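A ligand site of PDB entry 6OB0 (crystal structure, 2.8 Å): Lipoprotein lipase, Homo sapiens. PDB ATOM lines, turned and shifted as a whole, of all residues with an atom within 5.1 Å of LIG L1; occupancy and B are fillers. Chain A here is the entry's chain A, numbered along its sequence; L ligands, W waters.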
ATOM      1  N   TRP A  55      -3.954  22.274  18.119  1.00  0.00           N
ATOM      2  CA  TRP A  55      -3.217  21.075  17.734  1.00  0.00           C
ATOM      3  C   TRP A  55      -2.254  20.513  18.814  1.00  0.00           C
ATOM      4  O   TRP A  55      -1.534  21.254  19.505  1.00  0.00           O
ATOM      5  CB  TRP A  55      -2.444  21.315  16.433  1.00  0.00           C
ATOM      6  CG  TRP A  55      -2.066  20.028  15.771  1.00  0.00           C
ATOM      7  CD1 TRP A  55      -2.873  19.233  15.014  1.00  0.00           C
ATOM      8  CD2 TRP A  55      -0.800  19.379  15.837  1.00  0.00           C
ATOM      9  NE1 TRP A  55      -2.155  18.170  14.536  1.00  0.00           N
ATOM     10  CE2 TRP A  55      -0.895  18.212  15.062  1.00  0.00           C
ATOM     11  CE3 TRP A  55       0.439  19.717  16.423  1.00  0.00           C
ATOM     12  CZ2 TRP A  55       0.188  17.331  14.904  1.00  0.00           C
ATOM     13  CZ3 TRP A  55       1.492  18.826  16.295  1.00  0.00           C
ATOM     14  CH2 TRP A  55       1.368  17.649  15.552  1.00  0.00           C
ATOM     15  N   VAL A  57       0.388  16.966  19.643  1.00  0.00           N
ATOM     16  CA  VAL A  57       0.961  15.686  19.261  1.00  0.00           C
ATOM     17  C   VAL A  57       0.782  14.643  20.395  1.00  0.00           C
ATOM     18  O   VAL A  57       0.981  13.448  20.164  1.00  0.00           O
ATOM     19  CB  VAL A  57       2.437  15.908  18.858  1.00  0.00           C
ATOM     20  CG1 VAL A  57       3.399  15.816  20.062  1.00  0.00           C
ATOM     21  CG2 VAL A  57       2.846  14.985  17.714  1.00  0.00           C
ATOM     22  N   GLU A  92      -4.343  14.258  15.455  1.00  0.00           N
ATOM     23  CA  GLU A  92      -4.129  13.567  14.185  1.00  0.00           C
ATOM     24  C   GLU A  92      -3.024  14.274  13.427  1.00  0.00           C
ATOM     25  O   GLU A  92      -2.396  15.177  13.980  1.00  0.00           O
ATOM     26  CB  GLU A  92      -5.435  13.520  13.356  1.00  0.00           C
ATOM     27  CG  GLU A  92      -6.596  12.801  14.047  1.00  0.00           C
ATOM     28  CD  GLU A  92      -6.256  11.430  14.619  1.00  0.00           C
ATOM     29  OE1 GLU A  92      -6.447  11.232  15.844  1.00  0.00           O
ATOM     30  OE2 GLU A  92      -5.767  10.569  13.858  1.00  0.00           O
ATOM     31  N   HIS A  93      -2.733  13.861  12.182  1.00  0.00           N
ATOM     32  CA  HIS A  93      -1.735  14.489  11.314  1.00  0.00           C
ATOM     33  C   HIS A  93      -2.359  15.835  11.022  1.00  0.00           C
ATOM     34  O   HIS A  93      -3.584  15.945  10.843  1.00  0.00           O
ATOM     35  CB  HIS A  93      -1.499  13.636  10.040  1.00  0.00           C
ATOM     36  CG  HIS A  93      -0.780  14.301   8.893  1.00  0.00           C
ATOM     37  ND1 HIS A  93       0.434  14.946   9.068  1.00  0.00           N
ATOM     38  CD2 HIS A  93      -1.085  14.319   7.578  1.00  0.00           C
ATOM     39  CE1 HIS A  93       0.782  15.384   7.863  1.00  0.00           C
ATOM     40  NE2 HIS A  93      -0.102  15.027   6.942  1.00  0.00           N
ATOM     41  N   TYR A  94      -1.540  16.891  11.089  1.00  0.00           N
ATOM     42  CA  TYR A  94      -1.993  18.272  11.024  1.00  0.00           C
ATOM     43  C   TYR A  94      -3.111  18.511   9.988  1.00  0.00           C
ATOM     44  O   TYR A  94      -4.176  18.924  10.427  1.00  0.00           O
ATOM     45  CB  TYR A  94      -0.828  19.278  10.883  1.00  0.00           C
ATOM     46  CG  TYR A  94      -1.343  20.689  10.785  1.00  0.00           C
ATOM     47  CD1 TYR A  94      -1.745  21.388  11.921  1.00  0.00           C
ATOM     48  CD2 TYR A  94      -1.525  21.307   9.543  1.00  0.00           C
ATOM     49  CE1 TYR A  94      -2.279  22.676  11.827  1.00  0.00           C
ATOM     50  CE2 TYR A  94      -2.093  22.573   9.437  1.00  0.00           C
ATOM     51  CZ  TYR A  94      -2.419  23.273  10.579  1.00  0.00           C
ATOM     52  OH  TYR A  94      -2.947  24.551  10.469  1.00  0.00           O
ATOM     53  N   PRO A  95      -2.977  18.236   8.666  1.00  0.00           N
ATOM     54  CA  PRO A  95      -4.075  18.604   7.746  1.00  0.00           C
ATOM     55  C   PRO A  95      -5.405  17.921   8.031  1.00  0.00           C
ATOM     56  O   PRO A  95      -6.448  18.477   7.681  1.00  0.00           O
ATOM     57  CB  PRO A  95      -3.527  18.260   6.357  1.00  0.00           C
ATOM     58  CG  PRO A  95      -2.404  17.397   6.604  1.00  0.00           C
ATOM     59  CD  PRO A  95      -1.816  17.749   7.901  1.00  0.00           C
ATOM     60  N   TYR A 131      -7.284  28.953  20.646  1.00  0.00           N
ATOM     61  CA  TYR A 131      -5.837  28.926  20.408  1.00  0.00           C
ATOM     62  C   TYR A 131      -5.524  28.027  19.220  1.00  0.00           C
ATOM     63  O   TYR A 131      -6.151  26.978  19.082  1.00  0.00           O
ATOM     64  CB  TYR A 131      -5.151  28.356  21.662  1.00  0.00           C
ATOM     65  CG  TYR A 131      -3.665  28.118  21.521  1.00  0.00           C
ATOM     66  CD1 TYR A 131      -2.788  29.164  21.244  1.00  0.00           C
ATOM     67  CD2 TYR A 131      -3.139  26.841  21.616  1.00  0.00           C
ATOM     68  CE1 TYR A 131      -1.423  28.951  21.097  1.00  0.00           C
ATOM     69  CE2 TYR A 131      -1.773  26.613  21.503  1.00  0.00           C
ATOM     70  CZ  TYR A 131      -0.916  27.669  21.237  1.00  0.00           C
ATOM     71  OH  TYR A 131       0.432  27.431  21.111  1.00  0.00           O
ATOM     72  N   SER A 132      -4.506  28.400  18.405  1.00  0.00           N
ATOM     73  CA  SER A 132      -4.029  27.538  17.302  1.00  0.00           C
ATOM     74  C   SER A 132      -5.217  27.147  16.333  1.00  0.00           C
ATOM     75  O   SER A 132      -5.928  28.040  15.907  1.00  0.00           O
ATOM     76  CB  SER A 132      -3.260  26.349  17.921  1.00  0.00           C
ATOM     77  OG  SER A 132      -2.853  25.278  17.078  1.00  0.00           O
ATOM     78  N   LEU A 133      -5.505  25.846  16.082  1.00  0.00           N
ATOM     79  CA  LEU A 133      -6.680  25.432  15.296  1.00  0.00           C
ATOM     80  C   LEU A 133      -8.004  25.800  15.989  1.00  0.00           C
ATOM     81  O   LEU A 133      -8.995  26.025  15.316  1.00  0.00           O
ATOM     82  CB  LEU A 133      -6.675  23.929  15.007  1.00  0.00           C
ATOM     83  CG  LEU A 133      -5.524  23.367  14.171  1.00  0.00           C
ATOM     84  CD1 LEU A 133      -5.474  21.857  14.255  1.00  0.00           C
ATOM     85  CD2 LEU A 133      -5.593  23.844  12.702  1.00  0.00           C
ATOM     86  N   ASP A 156      -3.090  33.396  18.314  1.00  0.00           N
ATOM     87  CA  ASP A 156      -2.161  32.919  17.269  1.00  0.00           C
ATOM     88  C   ASP A 156      -2.831  31.839  16.382  1.00  0.00           C
ATOM     89  O   ASP A 156      -2.478  30.639  16.469  1.00  0.00           O
ATOM     90  CB  ASP A 156      -0.806  32.460  17.843  1.00  0.00           C
ATOM     91  CG  ASP A 156       0.353  32.807  16.916  1.00  0.00           C
ATOM     92  OD1 ASP A 156       0.320  33.889  16.303  1.00  0.00           O
ATOM     93  OD2 ASP A 156       1.283  31.980  16.809  1.00  0.00           O
ATOM     94  N   ALA A 158      -3.998  29.236  13.631  1.00  0.00           N
ATOM     95  CA  ALA A 158      -3.227  28.379  12.738  1.00  0.00           C
ATOM     96  C   ALA A 158      -3.174  28.963  11.331  1.00  0.00           C
ATOM     97  O   ALA A 158      -4.181  29.429  10.789  1.00  0.00           O
ATOM     98  CB  ALA A 158      -3.812  27.001  12.707  1.00  0.00           C
ATOM     99  N   GLY A 159      -1.964  28.983  10.788  1.00  0.00           N
ATOM    100  CA  GLY A 159      -1.684  29.520   9.457  1.00  0.00           C
ATOM    101  C   GLY A 159      -1.753  28.484   8.363  1.00  0.00           C
ATOM    102  O   GLY A 159      -2.462  28.701   7.378  1.00  0.00           O
ATOM    103  N   PRO A 160      -1.009  27.351   8.476  1.00  0.00           N
ATOM    104  CA  PRO A 160      -1.051  26.361   7.391  1.00  0.00           C
ATOM    105  C   PRO A 160      -2.456  25.895   7.112  1.00  0.00           C
ATOM    106  O   PRO A 160      -3.195  25.559   8.050  1.00  0.00           O
ATOM    107  CB  PRO A 160      -0.143  25.231   7.872  1.00  0.00           C
ATOM    108  CG  PRO A 160       0.719  25.853   8.922  1.00  0.00           C
ATOM    109  CD  PRO A 160      -0.108  26.902   9.561  1.00  0.00           C
ATOM    110  N   ASN A 161      -2.849  25.980   5.807  1.00  0.00           N
ATOM    111  CA  ASN A 161      -4.154  25.599   5.231  1.00  0.00           C
ATOM    112  C   ASN A 161      -5.292  26.548   5.624  1.00  0.00           C
ATOM    113  O   ASN A 161      -6.448  26.268   5.363  1.00  0.00           O
ATOM    114  CB  ASN A 161      -4.489  24.124   5.541  1.00  0.00           C
ATOM    115  CG  ASN A 161      -3.445  23.129   5.061  1.00  0.00           C
ATOM    116  OD1 ASN A 161      -2.617  23.400   4.165  1.00  0.00           O
ATOM    117  ND2 ASN A 161      -3.476  21.948   5.658  1.00  0.00           N
ATOM    118  N   ILE A 194       3.517  29.326  11.165  1.00  0.00           N
ATOM    119  CA  ILE A 194       2.668  28.541  12.093  1.00  0.00           C
ATOM    120  C   ILE A 194       1.438  29.381  12.500  1.00  0.00           C
ATOM    121  O   ILE A 194       0.308  28.868  12.542  1.00  0.00           O
ATOM    122  CB  ILE A 194       3.456  27.900  13.271  1.00  0.00           C
ATOM    123  CG1 ILE A 194       3.797  26.415  12.953  1.00  0.00           C
ATOM    124  CG2 ILE A 194       2.715  27.948  14.597  1.00  0.00           C
ATOM    125  CD1 ILE A 194       5.044  26.225  12.142  1.00  0.00           C
ATOM    126  N   LYS A 238       7.341  25.686  20.731  1.00  0.00           N
ATOM    127  CA  LYS A 238       6.092  26.491  20.614  1.00  0.00           C
ATOM    128  C   LYS A 238       6.079  27.772  21.498  1.00  0.00           C
ATOM    129  O   LYS A 238       4.994  28.144  21.929  1.00  0.00           O
ATOM    130  CB  LYS A 238       4.870  25.637  20.963  1.00  0.00           C
ATOM    131  CG  LYS A 238       4.393  24.753  19.852  1.00  0.00           C
ATOM    132  CD  LYS A 238       3.687  23.582  20.440  1.00  0.00           C
ATOM    133  CE  LYS A 238       2.237  23.798  20.761  1.00  0.00           C
ATOM    134  NZ  LYS A 238       1.496  22.518  20.578  1.00  0.00           N
ATOM    135  N   HIS A 241       4.469  31.086  19.643  1.00  0.00           N
ATOM    136  CA  HIS A 241       3.086  30.627  19.419  1.00  0.00           C
ATOM    137  C   HIS A 241       2.218  30.790  20.670  1.00  0.00           C
ATOM    138  O   HIS A 241       1.215  31.524  20.640  1.00  0.00           O
ATOM    139  CB  HIS A 241       3.106  29.145  18.987  1.00  0.00           C
ATOM    140  CG  HIS A 241       1.871  28.666  18.301  1.00  0.00           C
ATOM    141  ND1 HIS A 241       1.188  29.464  17.384  1.00  0.00           N
ATOM    142  CD2 HIS A 241       1.305  27.447  18.318  1.00  0.00           C
ATOM    143  CE1 HIS A 241       0.204  28.717  16.908  1.00  0.00           C
ATOM    144  NE2 HIS A 241       0.230  27.491  17.444  1.00  0.00           N
HETATM  145  C1  LIG L   1       2.922  18.816   8.590  1.00  0.00           C
HETATM  146  C2  LIG L   1       3.239  18.849   9.915  1.00  0.00           C
HETATM  147  C3  LIG L   1       2.056  21.149   8.178  1.00  0.00           C
HETATM  148  O1  LIG L   1       2.844  21.603   9.198  1.00  0.00           O
HETATM  149  O2  LIG L   1       4.133  16.664   9.738  1.00  0.00           O
HETATM  150  O3  LIG L   1      -0.967  26.086  15.420  1.00  0.00           O
HETATM  151  C4  LIG L   1       2.068  22.216  11.311  1.00  0.00           C
HETATM  152  C5  LIG L   1       1.813  21.961  12.681  1.00  0.00           C
HETATM  153  C6  LIG L   1       1.984  20.607  13.145  1.00  0.00           C
HETATM  154  C7  LIG L   1       2.480  19.600  12.276  1.00  0.00           C
HETATM  155  C8  LIG L   1       4.056  17.720  10.357  1.00  0.00           C
HETATM  156  C9  LIG L   1       1.169  23.042  13.467  1.00  0.00           C
HETATM  157  C10 LIG L   1       0.498  24.064  12.741  1.00  0.00           C
HETATM  158  C11 LIG L   1      -0.233  25.087  13.388  1.00  0.00           C
HETATM  159  C12 LIG L   1      -0.305  25.072  14.789  1.00  0.00           C
HETATM  160  C13 LIG L   1       0.335  24.058  15.533  1.00  0.00           C
HETATM  161  C14 LIG L   1       1.045  23.030  14.881  1.00  0.00           C
HETATM  162  C15 LIG L   1       5.617  17.074  12.219  1.00  0.00           C
HETATM  163  C16 LIG L   1       4.950  16.258  13.331  1.00  0.00           C
HETATM  164  C17 LIG L   1       3.056  14.864  13.996  1.00  0.00           C
HETATM  165  C18 LIG L   1       1.926  13.917  13.568  1.00  0.00           C
HETATM  166  C19 LIG L   1       3.072  13.383  11.527  1.00  0.00           C
HETATM  167  C20 LIG L   1       4.251  14.315  11.899  1.00  0.00           C
HETATM  168  C21 LIG L   1       0.226  24.027  16.965  1.00  0.00           C
HETATM  169  C22 LIG L   1       2.550  21.213  10.459  1.00  0.00           C
HETATM  170  C23 LIG L   1       2.105  19.781   7.825  1.00  0.00           C
HETATM  171  C24 LIG L   1       1.301  19.344   6.737  1.00  0.00           C
HETATM  172  C25 LIG L   1       0.507  20.280   6.024  1.00  0.00           C
HETATM  173  C26 LIG L   1       0.479  21.654   6.382  1.00  0.00           C
HETATM  174  C27 LIG L   1       1.273  22.086   7.457  1.00  0.00           C
HETATM  175  C28 LIG L   1       2.787  19.887  10.897  1.00  0.00           C
HETATM  176  N1  LIG L   1       4.703  17.954  11.514  1.00  0.00           N
HETATM  177  N2  LIG L   1       3.874  15.368  12.866  1.00  0.00           N
HETATM  178  N3  LIG L   1       0.098  23.990  18.106  1.00  0.00           N
HETATM  179  O4  LIG L   1       2.519  12.901  12.759  1.00  0.00           O
HETATM  180  C1  LG2 L   2       5.430  20.830  18.989  1.00  0.00           C
HETATM  181  C2  LG2 L   2       5.763  19.723  19.709  1.00  0.00           C
HETATM  182  C3  LG2 L   2       5.069  19.883  16.693  1.00  0.00           C
HETATM  183  O1  LG2 L   2       4.706  18.688  17.219  1.00  0.00           O
HETATM  184  O2  LG2 L   2       4.980  19.179  21.890  1.00  0.00           O
HETATM  185  O3  LG2 L   2       8.278  10.686  15.966  1.00  0.00           O
HETATM  186  C4  LG2 L   2       5.944  16.681  17.391  1.00  0.00           C
HETATM  187  C5  LG2 L   2       6.780  15.771  18.081  1.00  0.00           C
HETATM  188  C6  LG2 L   2       7.295  16.200  19.336  1.00  0.00           C
HETATM  189  C7  LG2 L   2       6.982  17.492  19.848  1.00  0.00           C
HETATM  190  C8  LG2 L   2       5.665  19.893  21.159  1.00  0.00           C
HETATM  191  C9  LG2 L   2       7.137  14.450  17.519  1.00  0.00           C
HETATM  192  C10 LG2 L   2       7.731  13.451  18.334  1.00  0.00           C
HETATM  193  C11 LG2 L   2       8.063  12.166  17.814  1.00  0.00           C
HETATM  194  C12 LG2 L   2       7.938  11.913  16.431  1.00  0.00           C
HETATM  195  C13 LG2 L   2       7.393  12.911  15.574  1.00  0.00           C
HETATM  196  C14 LG2 L   2       6.960  14.149  16.130  1.00  0.00           C
HETATM  197  C15 LG2 L   2       6.390  21.395  23.010  1.00  0.00           C
HETATM  198  C16 LG2 L   2       7.511  20.710  23.796  1.00  0.00           C
HETATM  199  C17 LG2 L   2       7.756  22.502  25.451  1.00  0.00           C
HETATM  200  C18 LG2 L   2       7.337  22.844  26.897  1.00  0.00           C
HETATM  201  C19 LG2 L   2       7.606  20.530  27.528  1.00  0.00           C
HETATM  202  C20 LG2 L   2       8.171  20.229  26.120  1.00  0.00           C
HETATM  203  C21 LG2 L   2       7.241  12.674  14.132  1.00  0.00           C
HETATM  204  C22 LG2 L   2       5.626  17.948  17.915  1.00  0.00           C
HETATM  205  C23 LG2 L   2       5.418  20.969  17.538  1.00  0.00           C
HETATM  206  C24 LG2 L   2       5.793  22.212  16.951  1.00  0.00           C
HETATM  207  C25 LG2 L   2       5.815  22.342  15.546  1.00  0.00           C
HETATM  208  C26 LG2 L   2       5.451  21.259  14.717  1.00  0.00           C
HETATM  209  C27 LG2 L   2       5.066  20.029  15.292  1.00  0.00           C
HETATM  210  C28 LG2 L   2       6.129  18.391  19.145  1.00  0.00           C
HETATM  211  N1  LG2 L   2       6.354  20.944  21.648  1.00  0.00           N
HETATM  212  N2  LG2 L   2       7.444  21.084  25.198  1.00  0.00           N
HETATM  213  N3  LG2 L   2       7.150  12.503  12.974  1.00  0.00           N
HETATM  214  O4  LG2 L   2       7.942  21.883  27.793  1.00  0.00           O
HETATM  215  O   HOH W   1       1.308  16.358  11.037  1.00  0.00           O
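An oxygen (O3) of LIG L1 lies within hydrogen-bond range of the side-chain hydroxyl of Ser 132. NE2 of His 241 is in hydrogen-bond range of O3 of LIG L1 (2.7 Å). The side-chain amino group (NZ) of Lys 238 lies within hydrogen-bond range of a nitrogen (N3) of LIG L1.
OG of Ser 132 sits at hydrogen-bond distance from N of Trp 55 (3.4 Å). The backbone carbonyl oxygen of Ser 132 lies within hydrogen-bond range of the backbone NH of Ala 158. The side-chain carboxylate (OD2) of Asp 156 sits at hydrogen-bond distance from a ring nitrogen (ND1) of His 241 (2.6 Å). NZ of Lys 238 lies within hydrogen-bond range of O of Trp 55 (3.5 Å). The backbone carbonyl oxygen of Pro 160 sits at hydrogen-bond distance from the side-chain hydroxyl of Tyr 94 (2.6 Å). The indole nitrogen (NE1) of Trp 55 is in hydrogen-bond range of the backbone carbonyl oxygen (O) of Glu 92. O of Ile 194 is in hydrogen-bond range of N of Gly 159, at 2.9 Å.
The backbone carbonyl oxygen of Trp 55 sits close to a nitrogen (N3) of LIG L1 (3.5 Å). Merely in contact with LIG L1: Val 57 (3.7 Å), His 93 (3.9 Å), Tyr 94 (3.2 Å), Pro 95 (3.7 Å), Pro 160 (3.5 Å) and Ile 194 (3.9 Å). The nearest printed residue that does not touch LIG L1 is Asn 161 (4.03 Å).
Water W1 lies within hydrogen-bond range of a ring nitrogen (ND1) of His 93 (2.6 Å), the backbone NH of Tyr 94 (2.9 Å) and an oxygen (O2) of LIG L1 (3.1 Å).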
